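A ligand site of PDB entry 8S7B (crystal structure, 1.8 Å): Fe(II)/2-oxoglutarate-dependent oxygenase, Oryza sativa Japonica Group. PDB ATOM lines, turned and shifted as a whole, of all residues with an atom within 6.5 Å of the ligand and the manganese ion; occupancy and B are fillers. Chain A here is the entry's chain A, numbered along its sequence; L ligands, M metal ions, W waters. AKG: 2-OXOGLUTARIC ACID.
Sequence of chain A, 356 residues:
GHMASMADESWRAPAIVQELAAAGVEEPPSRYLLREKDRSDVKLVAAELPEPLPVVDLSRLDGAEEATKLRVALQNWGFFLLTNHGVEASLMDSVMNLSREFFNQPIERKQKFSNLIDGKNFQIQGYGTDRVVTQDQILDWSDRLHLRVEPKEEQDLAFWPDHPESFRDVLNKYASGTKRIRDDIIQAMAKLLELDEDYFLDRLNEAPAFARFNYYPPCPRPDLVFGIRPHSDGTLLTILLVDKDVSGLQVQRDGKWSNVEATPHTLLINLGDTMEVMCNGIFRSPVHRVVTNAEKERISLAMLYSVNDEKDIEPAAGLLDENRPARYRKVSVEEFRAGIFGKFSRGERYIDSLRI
An oxygen (O3) of the ligand sits at hydrogen-bond distance from the side-chain hydroxyl (OG) of Ser 300.
The side-chain hydroxyl (OH) of Tyr 216 sits at hydrogen-bond distance from an oxygen (O3) of the ligand.
O3 of the ligand is in salt-bridge range of NH1 of Arg 298.
The side-chain amide nitrogen of Asn 214 lies within hydrogen-bond range of an oxygen (O2) of the ligand (3.0 Å).
O2 of the ligand is in salt-bridge range of NE of Arg 212 (3.7 Å).
The side-chain carboxylate (OD2) of Asp 233 lies within hydrogen-bond range of the side-chain hydroxyl (OG1) of Thr 238 (2.8 Å).
The side-chain carboxylate of Asp 233 is in hydrogen-bond range of the side-chain amide nitrogen of Asn 270 (3.1 Å).
The backbone carbonyl oxygen of Ser 300 is in hydrogen-bond range of the backbone NH of Asn 214.
The backbone NH of Tyr 216 sits at hydrogen-bond distance from the backbone carbonyl oxygen of Arg 298.
NE of Arg 212 is in hydrogen-bond range of OD1 of Asn 214 (2.8 Å).
The backbone carbonyl oxygen (O) of Ala 302 lies within hydrogen-bond range of the backbone NH (N) of Arg 212, 2.8 Å away.
The backbone NH of Val 290 sits at hydrogen-bond distance from the backbone carbonyl oxygen of Ile 228 (3.2 Å).
N of Leu 240 is in hydrogen-bond range of O of Leu 268, at 2.7 Å.
Leu 240 touches the ligand (CD2 to O4, 3.6 Å).
Val 242 touches the ligand (CG1 to O4, 3.7 Å).
CD1 of Leu 249 touches O4 of the ligand, at 3.8 Å.
Val 290 touches the ligand (CG2 to C5, 3.5 Å).
Ala 302 touches the ligand.
Hydrophobic or aromatic side chains within 4 Å of the ligand: Tyr 216, His 231, Leu 240, Val 242, Leu 249, His 288, Val 290 and Ala 302.
Within 4 Å of the ligand: Arg 212, Asn 214, Tyr 216, His 231, Asp 233, Leu 240, Val 242, Leu 249, His 288, Val 290, Arg 298, Ser 300 and Ala 302.
Along chain A the residues within 4 Å of the manganese ion span positions 231 to 288.
The manganese ion is bound by O1 of the ligand (2.1 Å), NE2 of His 288 (2.1 Å), O5 of the ligand (2.1 Å), NE2 of His 231 (2.1 Å), OD1 of Asp 233 (2.2 Å) and water W1 (2.3 Å).
The manganese ion has six donor atoms within binding distance.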
ATOM      1  N   ARG A 212      31.072  17.929  13.246  1.00  0.00           N
ATOM      2  CA  ARG A 212      31.748  18.110  14.526  1.00  0.00           C
ATOM      3  C   ARG A 212      30.961  17.373  15.593  1.00  0.00           C
ATOM      4  O   ARG A 212      29.894  17.831  16.015  1.00  0.00           O
ATOM      5  CB  ARG A 212      31.903  19.598  14.880  1.00  0.00           C
ATOM      6  CG  ARG A 212      32.704  19.852  16.161  1.00  0.00           C
ATOM      7  CD  ARG A 212      32.811  21.359  16.484  1.00  0.00           C
ATOM      8  NE  ARG A 212      33.462  21.557  17.782  1.00  0.00           N
ATOM      9  CZ  ARG A 212      34.680  22.037  17.957  1.00  0.00           C
ATOM     10  NH1 ARG A 212      35.406  22.480  16.949  1.00  0.00           N
ATOM     11  NH2 ARG A 212      35.194  22.063  19.185  1.00  0.00           N
ATOM     12  N   ASN A 214      30.730  16.757  19.185  1.00  0.00           N
ATOM     13  CA  ASN A 214      31.180  17.272  20.470  1.00  0.00           C
ATOM     14  C   ASN A 214      30.891  16.284  21.593  1.00  0.00           C
ATOM     15  O   ASN A 214      29.812  15.678  21.636  1.00  0.00           O
ATOM     16  CB  ASN A 214      30.494  18.598  20.797  1.00  0.00           C
ATOM     17  CG  ASN A 214      30.829  19.680  19.796  1.00  0.00           C
ATOM     18  OD1 ASN A 214      31.962  20.152  19.741  1.00  0.00           O
ATOM     19  ND2 ASN A 214      29.835  20.073  18.994  1.00  0.00           N
ATOM     20  N   TYR A 216      31.044  16.470  25.775  1.00  0.00           N
ATOM     21  CA  TYR A 216      31.234  17.273  26.980  1.00  0.00           C
ATOM     22  C   TYR A 216      31.212  16.357  28.191  1.00  0.00           C
ATOM     23  O   TYR A 216      30.126  15.939  28.628  1.00  0.00           O
ATOM     24  CB  TYR A 216      30.144  18.341  27.082  1.00  0.00           C
ATOM     25  CG  TYR A 216      29.976  19.177  25.833  1.00  0.00           C
ATOM     26  CD1 TYR A 216      30.734  20.329  25.642  1.00  0.00           C
ATOM     27  CD2 TYR A 216      29.076  18.816  24.842  1.00  0.00           C
ATOM     28  CE1 TYR A 216      30.612  21.090  24.497  1.00  0.00           C
ATOM     29  CE2 TYR A 216      28.927  19.585  23.685  1.00  0.00           C
ATOM     30  CZ  TYR A 216      29.701  20.713  23.519  1.00  0.00           C
ATOM     31  OH  TYR A 216      29.586  21.487  22.394  1.00  0.00           O
ATOM     32  N   ILE A 228      31.901  24.448  25.635  1.00  0.00           N
ATOM     33  CA  ILE A 228      32.502  25.150  24.501  1.00  0.00           C
ATOM     34  C   ILE A 228      32.297  26.633  24.717  1.00  0.00           C
ATOM     35  O   ILE A 228      31.224  27.069  25.164  1.00  0.00           O
ATOM     36  CB  ILE A 228      31.935  24.662  23.139  1.00  0.00           C
ATOM     37  CG1 ILE A 228      32.765  25.244  21.988  1.00  0.00           C
ATOM     38  CG2 ILE A 228      30.462  25.004  22.970  1.00  0.00           C
ATOM     39  CD1 ILE A 228      32.428  24.627  20.629  1.00  0.00           C
ATOM     40  N   HIS A 231      30.823  31.616  21.267  1.00  0.00           N
ATOM     41  CA  HIS A 231      31.307  31.791  19.915  1.00  0.00           C
ATOM     42  C   HIS A 231      30.108  31.909  18.993  1.00  0.00           C
ATOM     43  O   HIS A 231      29.007  31.467  19.316  1.00  0.00           O
ATOM     44  CB  HIS A 231      32.190  30.622  19.480  1.00  0.00           C
ATOM     45  CG  HIS A 231      31.436  29.339  19.274  1.00  0.00           C
ATOM     46  ND1 HIS A 231      31.062  28.518  20.317  1.00  0.00           N
ATOM     47  CD2 HIS A 231      30.966  28.756  18.144  1.00  0.00           C
ATOM     48  CE1 HIS A 231      30.401  27.480  19.835  1.00  0.00           C
ATOM     49  NE2 HIS A 231      30.318  27.603  18.527  1.00  0.00           N
ATOM     50  N   SER A 232      30.341  32.539  17.847  1.00  0.00           N
ATOM     51  CA  SER A 232      29.474  32.373  16.708  1.00  0.00           C
ATOM     52  C   SER A 232      30.159  31.426  15.734  1.00  0.00           C
ATOM     53  O   SER A 232      31.394  31.392  15.650  1.00  0.00           O
ATOM     54  CB  SER A 232      29.163  33.708  16.029  1.00  0.00           C
ATOM     55  OG  SER A 232      30.352  34.338  15.585  1.00  0.00           O
ATOM     56  N   ASP A 233      29.366  30.630  15.020  1.00  0.00           N
ATOM     57  CA  ASP A 233      29.946  29.768  14.008  1.00  0.00           C
ATOM     58  C   ASP A 233      30.438  30.602  12.829  1.00  0.00           C
ATOM     59  O   ASP A 233      29.866  31.648  12.497  1.00  0.00           O
ATOM     60  CB  ASP A 233      28.933  28.729  13.525  1.00  0.00           C
ATOM     61  CG  ASP A 233      28.543  27.735  14.614  1.00  0.00           C
ATOM     62  OD1 ASP A 233      29.230  27.667  15.661  1.00  0.00           O
ATOM     63  OD2 ASP A 233      27.550  27.006  14.418  1.00  0.00           O
ATOM     64  N   THR A 238      24.703  26.295  10.042  1.00  0.00           N
ATOM     65  CA  THR A 238      24.996  25.130  10.861  1.00  0.00           C
ATOM     66  C   THR A 238      23.698  24.408  11.174  1.00  0.00           C
ATOM     67  O   THR A 238      22.682  25.036  11.497  1.00  0.00           O
ATOM     68  CB  THR A 238      25.708  25.520  12.157  1.00  0.00           C
ATOM     69  OG1 THR A 238      26.954  26.166  11.859  1.00  0.00           O
ATOM     70  CG2 THR A 238      25.986  24.276  13.034  1.00  0.00           C
ATOM     71  N   LEU A 240      22.349  21.599  13.712  1.00  0.00           N
ATOM     72  CA  LEU A 240      22.826  21.050  14.977  1.00  0.00           C
ATOM     73  C   LEU A 240      21.832  20.046  15.539  1.00  0.00           C
ATOM     74  O   LEU A 240      20.625  20.320  15.599  1.00  0.00           O
ATOM     75  CB  LEU A 240      23.061  22.175  15.993  1.00  0.00           C
ATOM     76  CG  LEU A 240      23.549  21.807  17.393  1.00  0.00           C
ATOM     77  CD1 LEU A 240      24.959  21.286  17.338  1.00  0.00           C
ATOM     78  CD2 LEU A 240      23.462  23.019  18.327  1.00  0.00           C
ATOM     79  N   LEU A 241      22.348  18.902  15.983  1.00  0.00           N
ATOM     80  CA  LEU A 241      21.551  17.864  16.641  1.00  0.00           C
ATOM     81  C   LEU A 241      22.098  17.712  18.059  1.00  0.00           C
ATOM     82  O   LEU A 241      23.247  17.285  18.235  1.00  0.00           O
ATOM     83  CB  LEU A 241      21.623  16.545  15.875  1.00  0.00           C
ATOM     84  CG  LEU A 241      20.865  15.350  16.432  1.00  0.00           C
ATOM     85  CD1 LEU A 241      19.420  15.705  16.766  1.00  0.00           C
ATOM     86  CD2 LEU A 241      20.937  14.189  15.438  1.00  0.00           C
ATOM     87  N   VAL A 242      21.298  18.076  19.061  1.00  0.00           N
ATOM     88  CA  VAL A 242      21.778  18.118  20.433  1.00  0.00           C
ATOM     89  C   VAL A 242      21.373  16.844  21.166  1.00  0.00           C
ATOM     90  O   VAL A 242      20.430  16.136  20.788  1.00  0.00           O
ATOM     91  CB  VAL A 242      21.270  19.354  21.206  1.00  0.00           C
ATOM     92  CG1 VAL A 242      21.792  20.633  20.575  1.00  0.00           C
ATOM     93  CG2 VAL A 242      19.757  19.368  21.263  1.00  0.00           C
ATOM     94  N   ASP A 243      22.133  16.537  22.209  1.00  0.00           N
ATOM     95  CA  ASP A 243      21.783  15.530  23.194  1.00  0.00           C
ATOM     96  C   ASP A 243      20.308  15.629  23.569  1.00  0.00           C
ATOM     97  O   ASP A 243      19.817  16.710  23.896  1.00  0.00           O
ATOM     98  CB  ASP A 243      22.650  15.735  24.443  1.00  0.00           C
ATOM     99  CG  ASP A 243      22.767  14.504  25.310  1.00  0.00           C
ATOM    100  OD1 ASP A 243      21.736  13.961  25.765  1.00  0.00           O
ATOM    101  OD2 ASP A 243      23.918  14.086  25.538  1.00  0.00           O
ATOM    102  N   GLY A 248      22.425  22.045  28.086  1.00  0.00           N
ATOM    103  CA  GLY A 248      23.689  22.744  28.179  1.00  0.00           C
ATOM    104  C   GLY A 248      23.890  23.840  27.158  1.00  0.00           C
ATOM    105  O   GLY A 248      24.662  24.770  27.383  1.00  0.00           O
ATOM    106  N   LEU A 249      23.214  23.740  26.017  1.00  0.00           N
ATOM    107  CA  LEU A 249      23.328  24.779  24.999  1.00  0.00           C
ATOM    108  C   LEU A 249      22.647  26.063  25.468  1.00  0.00           C
ATOM    109  O   LEU A 249      21.524  26.032  25.985  1.00  0.00           O
ATOM    110  CB  LEU A 249      22.711  24.307  23.688  1.00  0.00           C
ATOM    111  CG  LEU A 249      22.688  25.295  22.527  1.00  0.00           C
ATOM    112  CD1 LEU A 249      24.098  25.704  22.120  1.00  0.00           C
ATOM    113  CD2 LEU A 249      21.937  24.707  21.339  1.00  0.00           C
ATOM    114  N   LEU A 268      18.205  22.016  15.276  1.00  0.00           N
ATOM    115  CA  LEU A 268      18.487  23.429  15.491  1.00  0.00           C
ATOM    116  C   LEU A 268      19.307  23.953  14.324  1.00  0.00           C
ATOM    117  O   LEU A 268      20.357  23.398  14.000  1.00  0.00           O
ATOM    118  CB  LEU A 268      19.232  23.654  16.801  1.00  0.00           C
ATOM    119  CG  LEU A 268      18.387  23.584  18.068  1.00  0.00           C
ATOM    120  CD1 LEU A 268      19.262  23.204  19.266  1.00  0.00           C
ATOM    121  CD2 LEU A 268      17.768  24.940  18.286  1.00  0.00           C
ATOM    122  N   ASN A 270      21.233  27.376  12.793  1.00  0.00           N
ATOM    123  CA  ASN A 270      21.696  28.737  13.051  1.00  0.00           C
ATOM    124  C   ASN A 270      22.527  29.211  11.871  1.00  0.00           C
ATOM    125  O   ASN A 270      23.218  28.429  11.216  1.00  0.00           O
ATOM    126  CB  ASN A 270      22.523  28.856  14.354  1.00  0.00           C
ATOM    127  CG  ASN A 270      23.793  28.014  14.340  1.00  0.00           C
ATOM    128  OD1 ASN A 270      23.747  26.811  14.574  1.00  0.00           O
ATOM    129  ND2 ASN A 270      24.933  28.665  14.106  1.00  0.00           N
ATOM    130  N   HIS A 288      26.732  31.602  20.903  1.00  0.00           N
ATOM    131  CA  HIS A 288      26.205  30.542  21.735  1.00  0.00           C
ATOM    132  C   HIS A 288      27.346  29.883  22.502  1.00  0.00           C
ATOM    133  O   HIS A 288      28.525  30.113  22.212  1.00  0.00           O
ATOM    134  CB  HIS A 288      25.440  29.497  20.905  1.00  0.00           C
ATOM    135  CG  HIS A 288      26.210  29.000  19.716  1.00  0.00           C
ATOM    136  ND1 HIS A 288      26.353  29.724  18.557  1.00  0.00           N
ATOM    137  CD2 HIS A 288      26.882  27.839  19.517  1.00  0.00           C
ATOM    138  CE1 HIS A 288      27.074  29.035  17.689  1.00  0.00           C
ATOM    139  NE2 HIS A 288      27.413  27.881  18.249  1.00  0.00           N
ATOM    140  N   ARG A 289      26.980  29.077  23.484  1.00  0.00           N
ATOM    141  CA  ARG A 289      27.971  28.377  24.310  1.00  0.00           C
ATOM    142  C   ARG A 289      27.314  27.121  24.876  1.00  0.00           C
ATOM    143  O   ARG A 289      26.107  26.925  24.779  1.00  0.00           O
ATOM    144  CB  ARG A 289      28.492  29.272  25.442  1.00  0.00           C
ATOM    145  CG  ARG A 289      27.462  29.507  26.545  1.00  0.00           C
ATOM    146  CD  ARG A 289      27.888  30.581  27.526  1.00  0.00           C
ATOM    147  NE  ARG A 289      26.933  30.713  28.618  1.00  0.00           N
ATOM    148  CZ  ARG A 289      27.018  31.632  29.570  1.00  0.00           C
ATOM    149  NH1 ARG A 289      28.003  32.512  29.603  1.00  0.00           N
ATOM    150  NH2 ARG A 289      26.082  31.663  30.513  1.00  0.00           N
ATOM    151  N   VAL A 290      28.136  26.265  25.478  1.00  0.00           N
ATOM    152  CA  VAL A 290      27.621  25.106  26.207  1.00  0.00           C
ATOM    153  C   VAL A 290      28.206  25.149  27.600  1.00  0.00           C
ATOM    154  O   VAL A 290      29.416  25.302  27.767  1.00  0.00           O
ATOM    155  CB  VAL A 290      27.966  23.777  25.513  1.00  0.00           C
ATOM    156  CG1 VAL A 290      27.611  22.593  26.404  1.00  0.00           C
ATOM    157  CG2 VAL A 290      27.220  23.679  24.190  1.00  0.00           C
ATOM    158  N   ARG A 298      27.497  14.915  27.834  1.00  0.00           N
ATOM    159  CA  ARG A 298      26.587  15.453  26.834  1.00  0.00           C
ATOM    160  C   ARG A 298      27.255  15.367  25.470  1.00  0.00           C
ATOM    161  O   ARG A 298      28.454  15.606  25.352  1.00  0.00           O
ATOM    162  CB  ARG A 298      26.212  16.915  27.142  1.00  0.00           C
ATOM    163  CG  ARG A 298      25.283  17.576  26.118  1.00  0.00           C
ATOM    164  CD  ARG A 298      24.999  19.038  26.476  1.00  0.00           C
ATOM    165  NE  ARG A 298      24.115  19.685  25.495  1.00  0.00           N
ATOM    166  CZ  ARG A 298      24.528  20.230  24.367  1.00  0.00           C
ATOM    167  NH1 ARG A 298      25.816  20.261  24.049  1.00  0.00           N
ATOM    168  NH2 ARG A 298      23.635  20.749  23.526  1.00  0.00           N
ATOM    169  N   ILE A 299      26.489  15.019  24.438  1.00  0.00           N
ATOM    170  CA  ILE A 299      27.025  14.966  23.088  1.00  0.00           C
ATOM    171  C   ILE A 299      26.185  15.843  22.172  1.00  0.00           C
ATOM    172  O   ILE A 299      25.009  16.114  22.451  1.00  0.00           O
ATOM    173  CB  ILE A 299      27.070  13.522  22.534  1.00  0.00           C
ATOM    174  CG1 ILE A 299      25.677  12.897  22.556  1.00  0.00           C
ATOM    175  CG2 ILE A 299      28.079  12.674  23.313  1.00  0.00           C
ATOM    176  CD1 ILE A 299      25.480  11.797  21.522  1.00  0.00           C
ATOM    177  N   SER A 300      26.800  16.316  21.102  1.00  0.00           N
ATOM    178  CA  SER A 300      26.064  16.986  20.031  1.00  0.00           C
ATOM    179  C   SER A 300      26.794  16.712  18.726  1.00  0.00           C
ATOM    180  O   SER A 300      27.969  16.331  18.717  1.00  0.00           O
ATOM    181  CB  SER A 300      25.947  18.492  20.268  1.00  0.00           C
ATOM    182  OG  SER A 300      27.218  19.108  20.153  1.00  0.00           O
ATOM    183  N   LEU A 301      26.082  16.900  17.616  1.00  0.00           N
ATOM    184  CA  LEU A 301      26.639  16.783  16.277  1.00  0.00           C
ATOM    185  C   LEU A 301      26.277  18.046  15.505  1.00  0.00           C
ATOM    186  O   LEU A 301      25.097  18.294  15.244  1.00  0.00           O
ATOM    187  CB  LEU A 301      26.118  15.540  15.551  1.00  0.00           C
ATOM    188  CG  LEU A 301      26.449  15.466  14.057  1.00  0.00           C
ATOM    189  CD1 LEU A 301      27.957  15.597  13.800  1.00  0.00           C
ATOM    190  CD2 LEU A 301      25.913  14.167  13.434  1.00  0.00           C
ATOM    191  N   ALA A 302      27.282  18.823  15.149  1.00  0.00           N
ATOM    192  CA  ALA A 302      27.088  20.027  14.339  1.00  0.00           C
ATOM    193  C   ALA A 302      27.539  19.742  12.913  1.00  0.00           C
ATOM    194  O   ALA A 302      28.693  19.371  12.692  1.00  0.00           O
ATOM    195  CB  ALA A 302      27.884  21.201  14.923  1.00  0.00           C
ATOM    196  N   LEU A 304      28.510  21.558   9.764  1.00  0.00           N
ATOM    197  CA  LEU A 304      29.039  22.899   9.533  1.00  0.00           C
ATOM    198  C   LEU A 304      29.196  23.100   8.037  1.00  0.00           C
ATOM    199  O   LEU A 304      30.058  22.472   7.413  1.00  0.00           O
ATOM    200  CB  LEU A 304      30.377  23.064  10.255  1.00  0.00           C
ATOM    201  CG  LEU A 304      30.329  22.824  11.759  1.00  0.00           C
ATOM    202  CD1 LEU A 304      31.727  22.508  12.306  1.00  0.00           C
ATOM    203  CD2 LEU A 304      29.739  24.043  12.470  1.00  0.00           C
HETATM  204  C1  AKG L   1      29.547  23.867  17.623  1.00  0.00           C
HETATM  205  O1  AKG L   1      29.905  24.813  16.919  1.00  0.00           O
HETATM  206  O2  AKG L   1      29.952  22.631  17.491  1.00  0.00           O
HETATM  207  C2  AKG L   1      28.557  24.086  18.753  1.00  0.00           C
HETATM  208  O5  AKG L   1      28.237  25.230  19.041  1.00  0.00           O
HETATM  209  C3  AKG L   1      28.006  22.887  19.483  1.00  0.00           C
HETATM  210  C4  AKG L   1      26.832  23.237  20.371  1.00  0.00           C
HETATM  211  C5  AKG L   1      26.341  22.090  21.214  1.00  0.00           C
HETATM  212  O3  AKG L   1      27.062  21.223  21.672  1.00  0.00           O
HETATM  213  O4  AKG L   1      25.044  22.140  21.426  1.00  0.00           O
HETATM  214 MN    MN M   1      28.824  26.510  17.436  1.00  0.00          MN
HETATM  215  O   HOH W   1      27.016  25.479  16.462  1.00  0.00           O
